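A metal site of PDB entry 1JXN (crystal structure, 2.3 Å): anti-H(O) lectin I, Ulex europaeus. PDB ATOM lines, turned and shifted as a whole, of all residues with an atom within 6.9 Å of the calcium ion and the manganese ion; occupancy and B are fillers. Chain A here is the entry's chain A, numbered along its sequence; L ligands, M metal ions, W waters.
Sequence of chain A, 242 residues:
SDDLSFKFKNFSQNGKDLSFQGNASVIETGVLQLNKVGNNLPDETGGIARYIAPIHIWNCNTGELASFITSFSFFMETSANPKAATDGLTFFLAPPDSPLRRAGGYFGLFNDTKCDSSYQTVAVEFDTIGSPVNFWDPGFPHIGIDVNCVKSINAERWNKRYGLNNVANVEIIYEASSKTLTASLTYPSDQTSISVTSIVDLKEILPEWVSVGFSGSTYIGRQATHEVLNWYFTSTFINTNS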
ATOM      1  N   ASP A  87      22.767 -13.958 -14.000  1.00  0.00           N
ATOM      2  CA  ASP A  87      22.145 -15.242 -14.364  1.00  0.00           C
ATOM      3  C   ASP A  87      20.690 -15.105 -13.968  1.00  0.00           C
ATOM      4  O   ASP A  87      19.847 -15.872 -14.430  1.00  0.00           O
ATOM      5  CB  ASP A  87      22.714 -16.363 -13.540  1.00  0.00           C
ATOM      6  CG  ASP A  87      23.974 -16.904 -14.106  1.00  0.00           C
ATOM      7  OD1 ASP A  87      25.060 -16.449 -13.685  1.00  0.00           O
ATOM      8  OD2 ASP A  87      23.888 -17.796 -14.984  1.00  0.00           O
ATOM      9  N   GLY A 104      25.789 -18.590  -9.873  1.00  0.00           N
ATOM     10  CA  GLY A 104      25.850 -18.544 -11.320  1.00  0.00           C
ATOM     11  C   GLY A 104      24.524 -19.036 -11.867  1.00  0.00           C
ATOM     12  O   GLY A 104      23.464 -18.554 -11.451  1.00  0.00           O
ATOM     13  N   GLY A 105      24.581 -19.998 -12.776  1.00  0.00           N
ATOM     14  CA  GLY A 105      23.365 -20.521 -13.371  1.00  0.00           C
ATOM     15  C   GLY A 105      22.535 -21.373 -12.443  1.00  0.00           C
ATOM     16  O   GLY A 105      21.386 -21.687 -12.738  1.00  0.00           O
ATOM     17  N   TYR A 106      23.115 -21.757 -11.318  1.00  0.00           N
ATOM     18  CA  TYR A 106      22.422 -22.592 -10.357  1.00  0.00           C
ATOM     19  C   TYR A 106      21.693 -21.802  -9.290  1.00  0.00           C
ATOM     20  O   TYR A 106      21.008 -22.380  -8.447  1.00  0.00           O
ATOM     21  CB  TYR A 106      23.393 -23.591  -9.761  1.00  0.00           C
ATOM     22  CG  TYR A 106      23.930 -24.531 -10.813  1.00  0.00           C
ATOM     23  CD1 TYR A 106      25.104 -24.218 -11.532  1.00  0.00           C
ATOM     24  CD2 TYR A 106      23.270 -25.724 -11.117  1.00  0.00           C
ATOM     25  CE1 TYR A 106      25.585 -25.079 -12.521  1.00  0.00           C
ATOM     26  CE2 TYR A 106      23.742 -26.577 -12.099  1.00  0.00           C
ATOM     27  CZ  TYR A 106      24.906 -26.249 -12.792  1.00  0.00           C
ATOM     28  OH  TYR A 106      25.382 -27.131 -13.709  1.00  0.00           O
ATOM     29  N   PHE A 107      21.839 -20.476  -9.330  1.00  0.00           N
ATOM     30  CA  PHE A 107      21.171 -19.545  -8.420  1.00  0.00           C
ATOM     31  C   PHE A 107      21.428 -19.633  -6.909  1.00  0.00           C
ATOM     32  O   PHE A 107      20.874 -18.843  -6.144  1.00  0.00           O
ATOM     33  CB  PHE A 107      19.660 -19.616  -8.654  1.00  0.00           C
ATOM     34  CG  PHE A 107      19.248 -19.279 -10.053  1.00  0.00           C
ATOM     35  CD1 PHE A 107      18.764 -20.269 -10.905  1.00  0.00           C
ATOM     36  CD2 PHE A 107      19.320 -17.958 -10.512  1.00  0.00           C
ATOM     37  CE1 PHE A 107      18.359 -19.959 -12.197  1.00  0.00           C
ATOM     38  CE2 PHE A 107      18.925 -17.632 -11.809  1.00  0.00           C
ATOM     39  CZ  PHE A 107      18.449 -18.626 -12.659  1.00  0.00           C
ATOM     40  N   GLU A 125      11.980 -19.127 -10.981  1.00  0.00           N
ATOM     41  CA  GLU A 125      13.136 -18.430 -11.492  1.00  0.00           C
ATOM     42  C   GLU A 125      12.855 -17.414 -12.593  1.00  0.00           C
ATOM     43  O   GLU A 125      11.846 -17.477 -13.285  1.00  0.00           O
ATOM     44  CB  GLU A 125      14.191 -19.421 -11.996  1.00  0.00           C
ATOM     45  CG  GLU A 125      13.728 -20.268 -13.168  1.00  0.00           C
ATOM     46  CD  GLU A 125      14.861 -20.870 -13.952  1.00  0.00           C
ATOM     47  OE1 GLU A 125      14.970 -20.563 -15.152  1.00  0.00           O
ATOM     48  OE2 GLU A 125      15.645 -21.664 -13.389  1.00  0.00           O
ATOM     49  N   PHE A 126      13.748 -16.438 -12.666  1.00  0.00           N
ATOM     50  CA  PHE A 126      13.730 -15.368 -13.655  1.00  0.00           C
ATOM     51  C   PHE A 126      15.161 -15.470 -14.163  1.00  0.00           C
ATOM     52  O   PHE A 126      16.080 -14.805 -13.658  1.00  0.00           O
ATOM     53  CB  PHE A 126      13.475 -14.024 -12.986  1.00  0.00           C
ATOM     54  CG  PHE A 126      12.189 -13.970 -12.228  1.00  0.00           C
ATOM     55  CD1 PHE A 126      12.071 -14.623 -10.996  1.00  0.00           C
ATOM     56  CD2 PHE A 126      11.073 -13.345 -12.756  1.00  0.00           C
ATOM     57  CE1 PHE A 126      10.869 -14.643 -10.313  1.00  0.00           C
ATOM     58  CE2 PHE A 126       9.863 -13.364 -12.085  1.00  0.00           C
ATOM     59  CZ  PHE A 126       9.767 -14.022 -10.860  1.00  0.00           C
ATOM     60  N   ASP A 127      15.346 -16.395 -15.100  1.00  0.00           N
ATOM     61  CA  ASP A 127      16.630 -16.721 -15.702  1.00  0.00           C
ATOM     62  C   ASP A 127      17.008 -15.775 -16.839  1.00  0.00           C
ATOM     63  O   ASP A 127      16.304 -15.699 -17.844  1.00  0.00           O
ATOM     64  CB  ASP A 127      16.552 -18.159 -16.226  1.00  0.00           C
ATOM     65  CG  ASP A 127      17.892 -18.781 -16.436  1.00  0.00           C
ATOM     66  OD1 ASP A 127      18.000 -20.010 -16.248  1.00  0.00           O
ATOM     67  OD2 ASP A 127      18.854 -18.067 -16.771  1.00  0.00           O
ATOM     68  N   THR A 128      18.125 -15.073 -16.701  1.00  0.00           N
ATOM     69  CA  THR A 128      18.547 -14.130 -17.737  1.00  0.00           C
ATOM     70  C   THR A 128      19.500 -14.679 -18.808  1.00  0.00           C
ATOM     71  O   THR A 128      19.743 -14.002 -19.797  1.00  0.00           O
ATOM     72  CB  THR A 128      19.149 -12.858 -17.124  1.00  0.00           C
ATOM     73  OG1 THR A 128      20.335 -13.198 -16.390  1.00  0.00           O
ATOM     74  CG2 THR A 128      18.165 -12.178 -16.179  1.00  0.00           C
ATOM     75  N   ILE A 129      20.064 -15.872 -18.588  1.00  0.00           N
ATOM     76  CA  ILE A 129      20.959 -16.464 -19.603  1.00  0.00           C
ATOM     77  C   ILE A 129      20.755 -17.984 -19.771  1.00  0.00           C
ATOM     78  O   ILE A 129      20.994 -18.783 -18.850  1.00  0.00           O
ATOM     79  CB  ILE A 129      22.452 -16.124 -19.353  1.00  0.00           C
ATOM     80  CG1 ILE A 129      23.217 -16.121 -20.682  1.00  0.00           C
ATOM     81  CG2 ILE A 129      23.106 -17.100 -18.386  1.00  0.00           C
ATOM     82  CD1 ILE A 129      22.871 -14.975 -21.621  1.00  0.00           C
ATOM     83  N   GLY A 130      20.276 -18.368 -20.957  1.00  0.00           N
ATOM     84  CA  GLY A 130      20.010 -19.769 -21.237  1.00  0.00           C
ATOM     85  C   GLY A 130      21.013 -20.388 -22.182  1.00  0.00           C
ATOM     86  O   GLY A 130      22.166 -19.930 -22.272  1.00  0.00           O
ATOM     87  N   SER A 131      20.593 -21.463 -22.860  1.00  0.00           N
ATOM     88  CA  SER A 131      21.425 -22.187 -23.839  1.00  0.00           C
ATOM     89  C   SER A 131      21.844 -21.258 -24.988  1.00  0.00           C
ATOM     90  O   SER A 131      21.058 -20.404 -25.413  1.00  0.00           O
ATOM     91  CB  SER A 131      20.647 -23.378 -24.406  1.00  0.00           C
ATOM     92  OG  SER A 131      21.523 -24.469 -24.658  1.00  0.00           O
ATOM     93  N   ASN A 134      24.100 -21.742 -20.904  1.00  0.00           N
ATOM     94  CA  ASN A 134      23.545 -22.575 -19.841  1.00  0.00           C
ATOM     95  C   ASN A 134      22.835 -23.703 -20.567  1.00  0.00           C
ATOM     96  O   ASN A 134      21.661 -23.609 -20.910  1.00  0.00           O
ATOM     97  CB  ASN A 134      22.538 -21.782 -18.993  1.00  0.00           C
ATOM     98  CG  ASN A 134      23.178 -21.108 -17.779  1.00  0.00           C
ATOM     99  OD1 ASN A 134      22.482 -20.507 -16.961  1.00  0.00           O
ATOM    100  ND2 ASN A 134      24.504 -21.211 -17.661  1.00  0.00           N
ATOM    101  N   TRP A 136      21.398 -26.678 -19.999  1.00  0.00           N
ATOM    102  CA  TRP A 136      20.099 -27.160 -19.491  1.00  0.00           C
ATOM    103  C   TRP A 136      18.878 -26.261 -19.677  1.00  0.00           C
ATOM    104  O   TRP A 136      17.759 -26.659 -19.319  1.00  0.00           O
ATOM    105  CB  TRP A 136      20.214 -27.446 -17.988  1.00  0.00           C
ATOM    106  CG  TRP A 136      20.630 -26.235 -17.201  1.00  0.00           C
ATOM    107  CD1 TRP A 136      19.800 -25.292 -16.635  1.00  0.00           C
ATOM    108  CD2 TRP A 136      21.961 -25.809 -16.906  1.00  0.00           C
ATOM    109  NE1 TRP A 136      20.543 -24.325 -16.007  1.00  0.00           N
ATOM    110  CE2 TRP A 136      21.872 -24.616 -16.149  1.00  0.00           C
ATOM    111  CE3 TRP A 136      23.231 -26.334 -17.199  1.00  0.00           C
ATOM    112  CZ2 TRP A 136      23.001 -23.943 -15.690  1.00  0.00           C
ATOM    113  CZ3 TRP A 136      24.351 -25.654 -16.732  1.00  0.00           C
ATOM    114  CH2 TRP A 136      24.227 -24.468 -15.985  1.00  0.00           C
ATOM    115  N   ASP A 137      19.098 -25.058 -20.191  1.00  0.00           N
ATOM    116  CA  ASP A 137      18.028 -24.074 -20.402  1.00  0.00           C
ATOM    117  C   ASP A 137      17.635 -23.861 -21.849  1.00  0.00           C
ATOM    118  O   ASP A 137      18.405 -24.179 -22.770  1.00  0.00           O
ATOM    119  CB  ASP A 137      18.491 -22.685 -19.968  1.00  0.00           C
ATOM    120  CG  ASP A 137      18.563 -22.519 -18.487  1.00  0.00           C
ATOM    121  OD1 ASP A 137      19.449 -21.751 -18.054  1.00  0.00           O
ATOM    122  OD2 ASP A 137      17.733 -23.104 -17.766  1.00  0.00           O
ATOM    123  N   PRO A 138      16.445 -23.283 -22.074  1.00  0.00           N
ATOM    124  CA  PRO A 138      15.994 -23.005 -23.431  1.00  0.00           C
ATOM    125  C   PRO A 138      16.946 -21.948 -24.013  1.00  0.00           C
ATOM    126  O   PRO A 138      17.780 -21.378 -23.296  1.00  0.00           O
ATOM    127  CB  PRO A 138      14.568 -22.443 -23.225  1.00  0.00           C
ATOM    128  CG  PRO A 138      14.512 -22.072 -21.784  1.00  0.00           C
ATOM    129  CD  PRO A 138      15.316 -23.149 -21.136  1.00  0.00           C
ATOM    130  N   HIS A 142      14.470 -16.333 -19.766  1.00  0.00           N
ATOM    131  CA  HIS A 142      13.109 -16.771 -19.481  1.00  0.00           C
ATOM    132  C   HIS A 142      12.776 -16.836 -17.988  1.00  0.00           C
ATOM    133  O   HIS A 142      13.613 -16.529 -17.119  1.00  0.00           O
ATOM    134  CB  HIS A 142      12.923 -18.179 -20.065  1.00  0.00           C
ATOM    135  CG  HIS A 142      13.844 -19.185 -19.469  1.00  0.00           C
ATOM    136  ND1 HIS A 142      15.216 -19.101 -19.535  1.00  0.00           N
ATOM    137  CD2 HIS A 142      13.579 -20.258 -18.685  1.00  0.00           C
ATOM    138  CE1 HIS A 142      15.739 -20.077 -18.790  1.00  0.00           C
ATOM    139  NE2 HIS A 142      14.788 -20.812 -18.254  1.00  0.00           N
ATOM    140  N   ILE A 143      11.538 -17.270 -17.730  1.00  0.00           N
ATOM    141  CA  ILE A 143      10.993 -17.445 -16.388  1.00  0.00           C
ATOM    142  C   ILE A 143      10.585 -18.919 -16.275  1.00  0.00           C
ATOM    143  O   ILE A 143      10.047 -19.484 -17.214  1.00  0.00           O
ATOM    144  CB  ILE A 143       9.791 -16.517 -16.211  1.00  0.00           C
ATOM    145  CG1 ILE A 143      10.293 -15.083 -16.037  1.00  0.00           C
ATOM    146  CG2 ILE A 143       8.901 -16.961 -15.043  1.00  0.00           C
ATOM    147  CD1 ILE A 143       9.210 -14.048 -16.086  1.00  0.00           C
ATOM    148  N   GLY A 144      10.868 -19.552 -15.146  1.00  0.00           N
ATOM    149  CA  GLY A 144      10.495 -20.938 -14.999  1.00  0.00           C
ATOM    150  C   GLY A 144      10.227 -21.392 -13.582  1.00  0.00           C
ATOM    151  O   GLY A 144      10.550 -20.694 -12.618  1.00  0.00           O
ATOM    152  N   ASP A 146      11.094 -24.220 -10.970  1.00  0.00           N
ATOM    153  CA  ASP A 146      12.092 -25.244 -10.684  1.00  0.00           C
ATOM    154  C   ASP A 146      11.648 -26.168  -9.559  1.00  0.00           C
ATOM    155  O   ASP A 146      11.464 -25.721  -8.432  1.00  0.00           O
ATOM    156  CB  ASP A 146      13.415 -24.617 -10.273  1.00  0.00           C
ATOM    157  CG  ASP A 146      14.011 -23.696 -11.324  1.00  0.00           C
ATOM    158  OD1 ASP A 146      13.356 -23.412 -12.341  1.00  0.00           O
ATOM    159  OD2 ASP A 146      15.154 -23.242 -11.092  1.00  0.00           O
ATOM    160  N   VAL A 150      17.589 -27.577 -11.298  1.00  0.00           N
ATOM    161  CA  VAL A 150      17.901 -26.311 -11.969  1.00  0.00           C
ATOM    162  C   VAL A 150      17.232 -26.205 -13.348  1.00  0.00           C
ATOM    163  O   VAL A 150      17.173 -25.119 -13.940  1.00  0.00           O
ATOM    164  CB  VAL A 150      19.416 -26.104 -12.139  1.00  0.00           C
ATOM    165  CG1 VAL A 150      19.976 -27.044 -13.190  1.00  0.00           C
ATOM    166  CG2 VAL A 150      19.697 -24.661 -12.451  1.00  0.00           C
ATOM    167  N   LYS A 151      16.749 -27.353 -13.820  1.00  0.00           N
ATOM    168  CA  LYS A 151      16.039 -27.465 -15.098  1.00  0.00           C
ATOM    169  C   LYS A 151      14.549 -27.346 -14.782  1.00  0.00           C
ATOM    170  O   LYS A 151      14.020 -28.148 -14.007  1.00  0.00           O
ATOM    171  CB  LYS A 151      16.325 -28.851 -15.698  1.00  0.00           C
ATOM    172  CG  LYS A 151      16.325 -28.917 -17.223  1.00  0.00           C
ATOM    173  CD  LYS A 151      16.762 -30.292 -17.711  1.00  0.00           C
ATOM    174  CE  LYS A 151      18.141 -30.698 -17.156  1.00  0.00           C
ATOM    175  NZ  LYS A 151      18.135 -31.110 -15.698  1.00  0.00           N
ATOM    176  N   SER A 152      13.868 -26.357 -15.370  1.00  0.00           N
ATOM    177  CA  SER A 152      12.442 -26.145 -15.129  1.00  0.00           C
ATOM    178  C   SER A 152      11.475 -27.249 -15.589  1.00  0.00           C
ATOM    179  O   SER A 152      11.819 -28.093 -16.442  1.00  0.00           O
ATOM    180  CB  SER A 152      12.004 -24.829 -15.762  1.00  0.00           C
ATOM    181  OG  SER A 152      12.825 -23.764 -15.348  1.00  0.00           O
ATOM    182  N   ALA A 155       8.524 -23.465 -18.625  1.00  0.00           N
ATOM    183  CA  ALA A 155       9.146 -22.137 -18.694  1.00  0.00           C
ATOM    184  C   ALA A 155       8.514 -21.225 -19.742  1.00  0.00           C
ATOM    185  O   ALA A 155       7.670 -21.669 -20.529  1.00  0.00           O
ATOM    186  CB  ALA A 155      10.637 -22.272 -18.951  1.00  0.00           C
HETATM  187  C1  LIG L   1      28.249 -21.527 -16.919  1.00  0.00           C
HETATM  188  C2  LIG L   1      27.595 -21.966 -15.581  1.00  0.00           C
HETATM  189  C3  LIG L   1      27.735 -20.779 -14.596  1.00  0.00           C
HETATM  190  C4  LIG L   1      27.038 -19.531 -15.196  1.00  0.00           C
HETATM  191  C5  LIG L   1      27.686 -19.174 -16.536  1.00  0.00           C
HETATM  192  C6  LIG L   1      26.999 -17.937 -17.153  1.00  0.00           C
HETATM  193  O1  LIG L   1      29.692 -21.299 -16.694  1.00  0.00           O
HETATM  194  O2  LIG L   1      28.224 -23.153 -15.093  1.00  0.00           O
HETATM  195  O3  LIG L   1      27.152 -21.123 -13.354  1.00  0.00           O
HETATM  196  O4  LIG L   1      25.647 -19.807 -15.401  1.00  0.00           O
HETATM  197  O5  LIG L   1      27.614 -20.298 -17.434  1.00  0.00           O
HETATM  198  C7  LIG L   1      30.811 -22.192 -16.451  1.00  0.00           C
HETATM  199 CA    CA M   1      20.179 -20.006 -16.799  1.00  0.00          CA
HETATM  200 MN    MN M   2      16.477 -21.712 -16.300  1.00  0.00          MN
HETATM  201  O   HOH W   1      14.751 -22.947 -16.772  1.00  0.00           O
HETATM  202  O   HOH W   2      20.247 -21.649 -15.111  1.00  0.00           O
HETATM  203  O   HOH W   3      17.742 -22.892 -14.926  1.00  0.00           O
HETATM  204  O   HOH W   4      21.245 -18.605 -15.418  1.00  0.00           O
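An oxygen (O4) of the ligand is in hydrogen-bond range of the side-chain amide nitrogen (ND2) of Asn 134 (2.9 Å).
N of Gly 105 is in hydrogen-bond range of O4 of the ligand (2.8 Å).
The side-chain carboxylate (OD2) of Asp 87 sits at hydrogen-bond distance from an oxygen (O4) of the ligand, 2.7 Å away.
OE1 of Glu 125 lies close to NE2 of His 142.
N of Glu 125 sits at hydrogen-bond distance from O of Gly 144 (2.7 Å).
N of Asp 127 sits at hydrogen-bond distance from O of His 142 (2.7 Å).
The side-chain carboxylate (OD1) of Asp 137 lies close to the indole nitrogen (NE1) of Trp 136, at 3.5 Å.
O of Asp 137 sits close to N of Ser 131 (3.5 Å).
Of the 24 residues printed, 4 come within 4 Å of the calcium ion.
The nearest printed residue that does not touch the manganese ion is Val 150 (4.2 Å).
Water W4 is bound to the calcium ion, at 2.2 Å.
The calcium ion is bound by OD1 of Asp 127 (2.2 Å).
The calcium ion is bound by OD1 of Asp 137, at 2.3 Å.
The calcium ion is bound by OD2 of Asp 127, 2.3 Å away.
The calcium ion is bound by water W2 (2.4 Å).
The calcium ion is bound by the side-chain amide oxygen (OD1) of Asn 134, 2.4 Å away.
The calcium ion is bound by the backbone carbonyl oxygen (O) of Ile 129, at 2.5 Å.
The calcium ion has seven donor atoms within binding distance.
Water W1 is bound to the manganese ion.
Water W3 binds the manganese ion (2.2 Å).
OE1 of Glu 125 binds the manganese ion (2.2 Å).
The manganese ion is bound by the side-chain carboxylate (OD1) of Asp 127 (2.3 Å).
The manganese ion is bound by the side-chain carboxylate (OD2) of Asp 137.
The manganese ion has five donor atoms within binding distance.
Slightly farther from the manganese ion lies NE2 of His 142 (2.7 Å).
Water W2 bridges the backbone carbonyl oxygen of Gly 105 (2.6 Å) and the indole nitrogen of Trp 136 (2.8 Å).
Water W1 bridges the side-chain hydroxyl (OG) of Ser 152 (2.5 Å) and a ring nitrogen (NE2) of His 142 (2.6 Å).
Water W3 lies within hydrogen-bond range of the backbone carbonyl oxygen of Val 150 (2.5 Å), the side-chain carboxylate of Glu 125 (2.9 Å) and the indole nitrogen of Trp 136 (3.3 Å).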
